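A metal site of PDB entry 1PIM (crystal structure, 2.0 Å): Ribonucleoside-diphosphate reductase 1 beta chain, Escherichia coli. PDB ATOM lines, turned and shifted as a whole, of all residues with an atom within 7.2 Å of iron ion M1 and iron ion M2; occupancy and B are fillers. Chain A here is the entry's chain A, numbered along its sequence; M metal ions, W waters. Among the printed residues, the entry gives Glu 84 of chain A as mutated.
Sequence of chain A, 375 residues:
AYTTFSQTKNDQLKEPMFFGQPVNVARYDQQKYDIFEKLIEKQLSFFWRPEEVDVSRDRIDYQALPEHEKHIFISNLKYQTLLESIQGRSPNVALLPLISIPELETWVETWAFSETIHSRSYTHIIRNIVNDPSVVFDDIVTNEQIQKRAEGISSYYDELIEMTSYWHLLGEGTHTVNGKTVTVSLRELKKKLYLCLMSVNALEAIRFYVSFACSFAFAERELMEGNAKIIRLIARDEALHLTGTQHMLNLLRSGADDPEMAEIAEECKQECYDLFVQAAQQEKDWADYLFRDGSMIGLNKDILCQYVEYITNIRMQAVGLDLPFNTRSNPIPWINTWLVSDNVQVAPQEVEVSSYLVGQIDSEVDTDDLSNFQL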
ATOM      1  N   GLN A  80     -21.483  27.601  -4.085  1.00  0.00           N
ATOM      2  CA  GLN A  80     -20.658  27.682  -2.895  1.00  0.00           C
ATOM      3  C   GLN A  80     -21.574  27.772  -1.668  1.00  0.00           C
ATOM      4  O   GLN A  80     -21.331  27.127  -0.637  1.00  0.00           O
ATOM      5  CB  GLN A  80     -19.738  28.909  -2.945  1.00  0.00           C
ATOM      6  CG  GLN A  80     -18.670  28.871  -4.054  1.00  0.00           C
ATOM      7  CD  GLN A  80     -17.887  30.175  -4.195  1.00  0.00           C
ATOM      8  OE1 GLN A  80     -18.469  31.251  -4.292  1.00  0.00           O
ATOM      9  NE2 GLN A  80     -16.556  30.073  -4.242  1.00  0.00           N
ATOM     10  N   LEU A  83     -23.180  24.377  -0.774  1.00  0.00           N
ATOM     11  CA  LEU A  83     -22.217  23.459  -0.179  1.00  0.00           C
ATOM     12  C   LEU A  83     -21.907  23.814   1.280  1.00  0.00           C
ATOM     13  O   LEU A  83     -21.754  22.935   2.129  1.00  0.00           O
ATOM     14  CB  LEU A  83     -20.929  23.430  -0.996  1.00  0.00           C
ATOM     15  CG  LEU A  83     -21.020  23.015  -2.472  1.00  0.00           C
ATOM     16  CD1 LEU A  83     -19.618  22.954  -3.067  1.00  0.00           C
ATOM     17  CD2 LEU A  83     -21.707  21.667  -2.611  1.00  0.00           C
ATOM     18  N   GLU A  84     -21.818  25.114   1.577  1.00  0.00           N
ATOM     19  CA  GLU A  84     -21.517  25.550   2.934  1.00  0.00           C
ATOM     20  C   GLU A  84     -22.728  25.355   3.840  1.00  0.00           C
ATOM     21  O   GLU A  84     -22.572  25.117   5.041  1.00  0.00           O
ATOM     22  CB  GLU A  84     -21.076  27.019   2.937  1.00  0.00           C
ATOM     23  CG  GLU A  84     -19.875  27.284   2.039  1.00  0.00           C
ATOM     24  CD  GLU A  84     -18.537  26.985   2.704  1.00  0.00           C
ATOM     25  OE1 GLU A  84     -18.473  26.101   3.584  1.00  0.00           O
ATOM     26  OE2 GLU A  84     -17.537  27.633   2.322  1.00  0.00           O
ATOM     27  N   GLN A  87     -22.384  21.839   4.784  1.00  0.00           N
ATOM     28  CA  GLN A  87     -21.189  21.646   5.618  1.00  0.00           C
ATOM     29  C   GLN A  87     -21.283  22.282   6.998  1.00  0.00           C
ATOM     30  O   GLN A  87     -20.588  21.898   7.924  1.00  0.00           O
ATOM     31  CB  GLN A  87     -19.940  22.172   4.902  1.00  0.00           C
ATOM     32  CG  GLN A  87     -19.404  21.261   3.802  1.00  0.00           C
ATOM     33  CD  GLN A  87     -19.032  19.869   4.322  1.00  0.00           C
ATOM     34  OE1 GLN A  87     -19.847  18.946   4.324  1.00  0.00           O
ATOM     35  NE2 GLN A  87     -17.795  19.731   4.791  1.00  0.00           N
ATOM     36  N   TRP A 111     -14.454  22.758  13.069  1.00  0.00           N
ATOM     37  CA  TRP A 111     -14.539  22.704  11.611  1.00  0.00           C
ATOM     38  C   TRP A 111     -15.929  23.149  11.156  1.00  0.00           C
ATOM     39  O   TRP A 111     -16.057  24.001  10.280  1.00  0.00           O
ATOM     40  CB  TRP A 111     -14.206  21.267  11.184  1.00  0.00           C
ATOM     41  CG  TRP A 111     -14.578  20.825   9.815  1.00  0.00           C
ATOM     42  CD1 TRP A 111     -14.741  21.606   8.706  1.00  0.00           C
ATOM     43  CD2 TRP A 111     -14.725  19.470   9.375  1.00  0.00           C
ATOM     44  NE1 TRP A 111     -14.984  20.810   7.596  1.00  0.00           N
ATOM     45  CE2 TRP A 111     -14.979  19.505   7.986  1.00  0.00           C
ATOM     46  CE3 TRP A 111     -14.672  18.225  10.030  1.00  0.00           C
ATOM     47  CZ2 TRP A 111     -15.172  18.332   7.234  1.00  0.00           C
ATOM     48  CZ3 TRP A 111     -14.862  17.064   9.272  1.00  0.00           C
ATOM     49  CH2 TRP A 111     -15.114  17.133   7.889  1.00  0.00           C
ATOM     50  N   SER A 114     -16.474  26.861  11.675  1.00  0.00           N
ATOM     51  CA  SER A 114     -15.844  27.664  10.632  1.00  0.00           C
ATOM     52  C   SER A 114     -16.699  27.684   9.371  1.00  0.00           C
ATOM     53  O   SER A 114     -16.718  28.680   8.648  1.00  0.00           O
ATOM     54  CB  SER A 114     -14.416  27.152  10.314  1.00  0.00           C
ATOM     55  OG  SER A 114     -14.432  25.912   9.644  1.00  0.00           O
ATOM     56  N   GLU A 115     -17.455  26.613   9.108  1.00  0.00           N
ATOM     57  CA  GLU A 115     -18.317  26.573   7.935  1.00  0.00           C
ATOM     58  C   GLU A 115     -19.457  27.593   8.066  1.00  0.00           C
ATOM     59  O   GLU A 115     -19.836  28.212   7.067  1.00  0.00           O
ATOM     60  CB  GLU A 115     -18.893  25.166   7.712  1.00  0.00           C
ATOM     61  CG  GLU A 115     -17.849  24.072   7.579  1.00  0.00           C
ATOM     62  CD  GLU A 115     -16.983  24.216   6.333  1.00  0.00           C
ATOM     63  OE1 GLU A 115     -16.928  25.322   5.773  1.00  0.00           O
ATOM     64  OE2 GLU A 115     -16.361  23.220   5.914  1.00  0.00           O
ATOM     65  N   THR A 116     -19.996  27.784   9.269  1.00  0.00           N
ATOM     66  CA  THR A 116     -21.088  28.734   9.411  1.00  0.00           C
ATOM     67  C   THR A 116     -20.563  30.152   9.182  1.00  0.00           C
ATOM     68  O   THR A 116     -21.314  31.055   8.809  1.00  0.00           O
ATOM     69  CB  THR A 116     -21.810  28.660  10.810  1.00  0.00           C
ATOM     70  OG1 THR A 116     -20.944  29.138  11.844  1.00  0.00           O
ATOM     71  CG2 THR A 116     -22.237  27.219  11.105  1.00  0.00           C
ATOM     72  N   ILE A 117     -19.262  30.354   9.405  1.00  0.00           N
ATOM     73  CA  ILE A 117     -18.659  31.652   9.163  1.00  0.00           C
ATOM     74  C   ILE A 117     -18.602  31.862   7.640  1.00  0.00           C
ATOM     75  O   ILE A 117     -18.860  32.961   7.148  1.00  0.00           O
ATOM     76  CB  ILE A 117     -17.238  31.739   9.756  1.00  0.00           C
ATOM     77  CG1 ILE A 117     -17.310  31.664  11.285  1.00  0.00           C
ATOM     78  CG2 ILE A 117     -16.539  33.021   9.278  1.00  0.00           C
ATOM     79  CD1 ILE A 117     -18.140  32.789  11.938  1.00  0.00           C
ATOM     80  N   HIS A 118     -18.261  30.800   6.914  1.00  0.00           N
ATOM     81  CA  HIS A 118     -18.198  30.887   5.457  1.00  0.00           C
ATOM     82  C   HIS A 118     -19.587  31.200   4.911  1.00  0.00           C
ATOM     83  O   HIS A 118     -19.739  32.096   4.065  1.00  0.00           O
ATOM     84  CB  HIS A 118     -17.639  29.583   4.866  1.00  0.00           C
ATOM     85  CG  HIS A 118     -16.227  29.296   5.277  1.00  0.00           C
ATOM     86  ND1 HIS A 118     -15.593  28.109   4.984  1.00  0.00           N
ATOM     87  CD2 HIS A 118     -15.324  30.053   5.942  1.00  0.00           C
ATOM     88  CE1 HIS A 118     -14.361  28.146   5.463  1.00  0.00           C
ATOM     89  NE2 HIS A 118     -14.178  29.316   6.054  1.00  0.00           N
ATOM     90  N   SER A 119     -20.615  30.490   5.401  1.00  0.00           N
ATOM     91  CA  SER A 119     -21.989  30.732   4.965  1.00  0.00           C
ATOM     92  C   SER A 119     -22.338  32.188   5.207  1.00  0.00           C
ATOM     93  O   SER A 119     -22.966  32.836   4.362  1.00  0.00           O
ATOM     94  CB  SER A 119     -22.974  29.835   5.723  1.00  0.00           C
ATOM     95  OG  SER A 119     -22.777  28.469   5.426  1.00  0.00           O
ATOM     96  N   TYR A 122     -20.937  34.590   2.661  1.00  0.00           N
ATOM     97  CA  TYR A 122     -21.666  34.656   1.390  1.00  0.00           C
ATOM     98  C   TYR A 122     -22.900  35.568   1.467  1.00  0.00           C
ATOM     99  O   TYR A 122     -23.271  36.176   0.464  1.00  0.00           O
ATOM    100  CB  TYR A 122     -22.077  33.258   0.931  1.00  0.00           C
ATOM    101  CG  TYR A 122     -20.897  32.379   0.562  1.00  0.00           C
ATOM    102  CD1 TYR A 122     -19.915  32.832  -0.318  1.00  0.00           C
ATOM    103  CD2 TYR A 122     -20.747  31.109   1.113  1.00  0.00           C
ATOM    104  CE1 TYR A 122     -18.816  32.051  -0.640  1.00  0.00           C
ATOM    105  CE2 TYR A 122     -19.646  30.308   0.801  1.00  0.00           C
ATOM    106  CZ  TYR A 122     -18.691  30.786  -0.075  1.00  0.00           C
ATOM    107  OH  TYR A 122     -17.598  29.997  -0.382  1.00  0.00           O
ATOM    108  N   LEU A 203     -15.534  16.772  -1.623  1.00  0.00           N
ATOM    109  CA  LEU A 203     -16.244  18.048  -1.599  1.00  0.00           C
ATOM    110  C   LEU A 203     -15.319  19.234  -1.316  1.00  0.00           C
ATOM    111  O   LEU A 203     -15.339  20.234  -2.031  1.00  0.00           O
ATOM    112  CB  LEU A 203     -17.374  17.998  -0.570  1.00  0.00           C
ATOM    113  CG  LEU A 203     -18.221  19.255  -0.334  1.00  0.00           C
ATOM    114  CD1 LEU A 203     -18.738  19.812  -1.649  1.00  0.00           C
ATOM    115  CD2 LEU A 203     -19.384  18.920   0.586  1.00  0.00           C
ATOM    116  N   GLU A 204     -14.497  19.122  -0.278  1.00  0.00           N
ATOM    117  CA  GLU A 204     -13.604  20.230   0.097  1.00  0.00           C
ATOM    118  C   GLU A 204     -12.279  20.305  -0.653  1.00  0.00           C
ATOM    119  O   GLU A 204     -11.698  21.388  -0.786  1.00  0.00           O
ATOM    120  CB  GLU A 204     -13.344  20.177   1.600  1.00  0.00           C
ATOM    121  CG  GLU A 204     -14.624  20.287   2.423  1.00  0.00           C
ATOM    122  CD  GLU A 204     -14.370  20.241   3.921  1.00  0.00           C
ATOM    123  OE1 GLU A 204     -13.648  19.327   4.374  1.00  0.00           O
ATOM    124  OE2 GLU A 204     -14.912  21.109   4.630  1.00  0.00           O
ATOM    125  N   PHE A 208     -14.712  22.578  -4.024  1.00  0.00           N
ATOM    126  CA  PHE A 208     -14.474  23.940  -3.592  1.00  0.00           C
ATOM    127  C   PHE A 208     -13.324  24.636  -4.302  1.00  0.00           C
ATOM    128  O   PHE A 208     -13.381  25.830  -4.564  1.00  0.00           O
ATOM    129  CB  PHE A 208     -14.277  24.001  -2.081  1.00  0.00           C
ATOM    130  CG  PHE A 208     -15.512  24.390  -1.339  1.00  0.00           C
ATOM    131  CD1 PHE A 208     -16.086  25.651  -1.532  1.00  0.00           C
ATOM    132  CD2 PHE A 208     -16.146  23.496  -0.490  1.00  0.00           C
ATOM    133  CE1 PHE A 208     -17.267  26.007  -0.900  1.00  0.00           C
ATOM    134  CE2 PHE A 208     -17.339  23.834   0.150  1.00  0.00           C
ATOM    135  CZ  PHE A 208     -17.895  25.101  -0.054  1.00  0.00           C
ATOM    136  N   PHE A 212     -13.036  28.312  -6.457  1.00  0.00           N
ATOM    137  CA  PHE A 212     -12.065  29.357  -6.159  1.00  0.00           C
ATOM    138  C   PHE A 212     -11.451  29.891  -7.454  1.00  0.00           C
ATOM    139  O   PHE A 212     -11.185  31.086  -7.572  1.00  0.00           O
ATOM    140  CB  PHE A 212     -10.920  28.814  -5.277  1.00  0.00           C
ATOM    141  CG  PHE A 212     -11.366  28.292  -3.944  1.00  0.00           C
ATOM    142  CD1 PHE A 212     -12.492  28.820  -3.310  1.00  0.00           C
ATOM    143  CD2 PHE A 212     -10.645  27.295  -3.297  1.00  0.00           C
ATOM    144  CE1 PHE A 212     -12.884  28.364  -2.047  1.00  0.00           C
ATOM    145  CE2 PHE A 212     -11.021  26.833  -2.039  1.00  0.00           C
ATOM    146  CZ  PHE A 212     -12.144  27.373  -1.411  1.00  0.00           C
ATOM    147  N   ILE A 234     -11.294  32.040   3.049  1.00  0.00           N
ATOM    148  CA  ILE A 234     -12.010  30.769   3.059  1.00  0.00           C
ATOM    149  C   ILE A 234     -11.048  29.655   2.610  1.00  0.00           C
ATOM    150  O   ILE A 234     -10.968  28.599   3.239  1.00  0.00           O
ATOM    151  CB  ILE A 234     -13.252  30.825   2.116  1.00  0.00           C
ATOM    152  CG1 ILE A 234     -14.311  31.757   2.722  1.00  0.00           C
ATOM    153  CG2 ILE A 234     -13.829  29.423   1.901  1.00  0.00           C
ATOM    154  CD1 ILE A 234     -15.526  31.967   1.829  1.00  0.00           C
ATOM    155  N   ASP A 237      -8.811  28.369   5.169  1.00  0.00           N
ATOM    156  CA  ASP A 237      -9.436  27.447   6.115  1.00  0.00           C
ATOM    157  C   ASP A 237      -9.619  26.080   5.467  1.00  0.00           C
ATOM    158  O   ASP A 237      -9.308  25.054   6.069  1.00  0.00           O
ATOM    159  CB  ASP A 237     -10.812  27.946   6.565  1.00  0.00           C
ATOM    160  CG  ASP A 237     -10.745  29.230   7.370  1.00  0.00           C
ATOM    161  OD1 ASP A 237      -9.831  29.387   8.193  1.00  0.00           O
ATOM    162  OD2 ASP A 237     -11.648  30.078   7.191  1.00  0.00           O
ATOM    163  N   GLU A 238     -10.129  26.079   4.229  1.00  0.00           N
ATOM    164  CA  GLU A 238     -10.381  24.836   3.502  1.00  0.00           C
ATOM    165  C   GLU A 238      -9.175  23.895   3.435  1.00  0.00           C
ATOM    166  O   GLU A 238      -9.351  22.679   3.421  1.00  0.00           O
ATOM    167  CB  GLU A 238     -10.862  25.132   2.080  1.00  0.00           C
ATOM    168  CG  GLU A 238     -12.286  25.648   2.040  1.00  0.00           C
ATOM    169  CD  GLU A 238     -13.233  24.780   2.859  1.00  0.00           C
ATOM    170  OE1 GLU A 238     -13.249  23.547   2.621  1.00  0.00           O
ATOM    171  OE2 GLU A 238     -13.943  25.321   3.740  1.00  0.00           O
ATOM    172  N   ALA A 239      -7.978  24.469   3.395  1.00  0.00           N
ATOM    173  CA  ALA A 239      -6.754  23.670   3.349  1.00  0.00           C
ATOM    174  C   ALA A 239      -6.614  22.899   4.667  1.00  0.00           C
ATOM    175  O   ALA A 239      -6.083  21.774   4.688  1.00  0.00           O
ATOM    176  CB  ALA A 239      -5.547  24.593   3.138  1.00  0.00           C
ATOM    177  N   LEU A 240      -7.071  23.506   5.759  1.00  0.00           N
ATOM    178  CA  LEU A 240      -7.024  22.833   7.052  1.00  0.00           C
ATOM    179  C   LEU A 240      -8.061  21.705   7.084  1.00  0.00           C
ATOM    180  O   LEU A 240      -7.780  20.605   7.570  1.00  0.00           O
ATOM    181  CB  LEU A 240      -7.345  23.814   8.205  1.00  0.00           C
ATOM    182  CG  LEU A 240      -6.376  24.961   8.529  1.00  0.00           C
ATOM    183  CD1 LEU A 240      -6.873  25.699   9.774  1.00  0.00           C
ATOM    184  CD2 LEU A 240      -4.986  24.400   8.792  1.00  0.00           C
ATOM    185  N   HIS A 241      -9.252  21.985   6.584  1.00  0.00           N
ATOM    186  CA  HIS A 241     -10.322  20.989   6.574  1.00  0.00           C
ATOM    187  C   HIS A 241      -9.963  19.752   5.759  1.00  0.00           C
ATOM    188  O   HIS A 241     -10.176  18.627   6.217  1.00  0.00           O
ATOM    189  CB  HIS A 241     -11.616  21.591   6.010  1.00  0.00           C
ATOM    190  CG  HIS A 241     -12.074  22.827   6.724  1.00  0.00           C
ATOM    191  ND1 HIS A 241     -13.150  23.586   6.294  1.00  0.00           N
ATOM    192  CD2 HIS A 241     -11.590  23.456   7.821  1.00  0.00           C
ATOM    193  CE1 HIS A 241     -13.302  24.617   7.098  1.00  0.00           C
ATOM    194  NE2 HIS A 241     -12.372  24.573   8.029  1.00  0.00           N
ATOM    195  N   LEU A 242      -9.405  19.956   4.569  1.00  0.00           N
ATOM    196  CA  LEU A 242      -9.058  18.823   3.732  1.00  0.00           C
ATOM    197  C   LEU A 242      -7.908  18.030   4.345  1.00  0.00           C
ATOM    198  O   LEU A 242      -7.799  16.828   4.116  1.00  0.00           O
ATOM    199  CB  LEU A 242      -8.705  19.284   2.308  1.00  0.00           C
ATOM    200  CG  LEU A 242      -7.400  20.027   2.040  1.00  0.00           C
ATOM    201  CD1 LEU A 242      -6.258  19.020   1.903  1.00  0.00           C
ATOM    202  CD2 LEU A 242      -7.536  20.835   0.749  1.00  0.00           C
HETATM  203 FE    FE M   1     -14.569  23.258   4.565  1.00  0.00          FE
HETATM  204 FE    FE M   2     -16.255  26.190   3.935  1.00  0.00          FE
HETATM  205  O   HOH W   1     -16.057  23.405   2.939  1.00  0.00           O
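A ring nitrogen (NE2) of His 118 sits at hydrogen-bond distance from the side-chain carboxylate (OD2) of Asp 237, at 2.9 Å. NE2 of His 241 is in hydrogen-bond range of OG of Ser 114 (2.9 Å). O of Glu 115 lies within hydrogen-bond range of OG of Ser 119, at 3.4 Å. O of Glu 84 sits close to OG of Ser 119 (3.4 Å). NE2 of Gln 87 sits close to OE2 of Glu 204. OE2 of Glu 204 lies close to NE1 of Trp 111 (3.0 Å). The side-chain hydroxyl (OG) of Ser 114 is in hydrogen-bond range of the backbone carbonyl oxygen (O) of Trp 111 (2.6 Å). The indole nitrogen (NE1) of Trp 111 lies close to the side-chain carboxylate (OE2) of Glu 115, 3.2 Å away.
Merely in contact with iron ion M1: Trp 111 (3.9 Å). Five residues have an atom within 4 Å of iron ion M1: Trp 111, Glu 115, Glu 204, Glu 238 and His 241. The nearest printed residue that does not touch iron ion M1 is Gln 87 (4.8 Å).
The nearest printed residue that does not touch iron ion M2 is Phe 208 (4.4 Å).
Iron ion M1 is bound by OE2 of Glu 204 (2.2 Å). Iron ion M1 is bound by water W1, at 2.2 Å. The side-chain carboxylate (OE2) of Glu 115 binds iron ion M1 (2.2 Å). Iron ion M1 is bound by a ring nitrogen (ND1) of His 241, at 2.3 Å. OE2 of Glu 238 binds iron ion M1. OE1 of Glu 238 binds iron ion M1 (2.4 Å). Iron ion M1 has six donor atoms within binding distance.
Iron ion M2 is bound by OE1 of Glu 115 (2.1 Å), OE1 of Glu 84 (2.2 Å), ND1 of His 118 (2.3 Å), OE2 of Glu 238 (2.5 Å) and OE2 of Glu 84 (2.5 Å).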
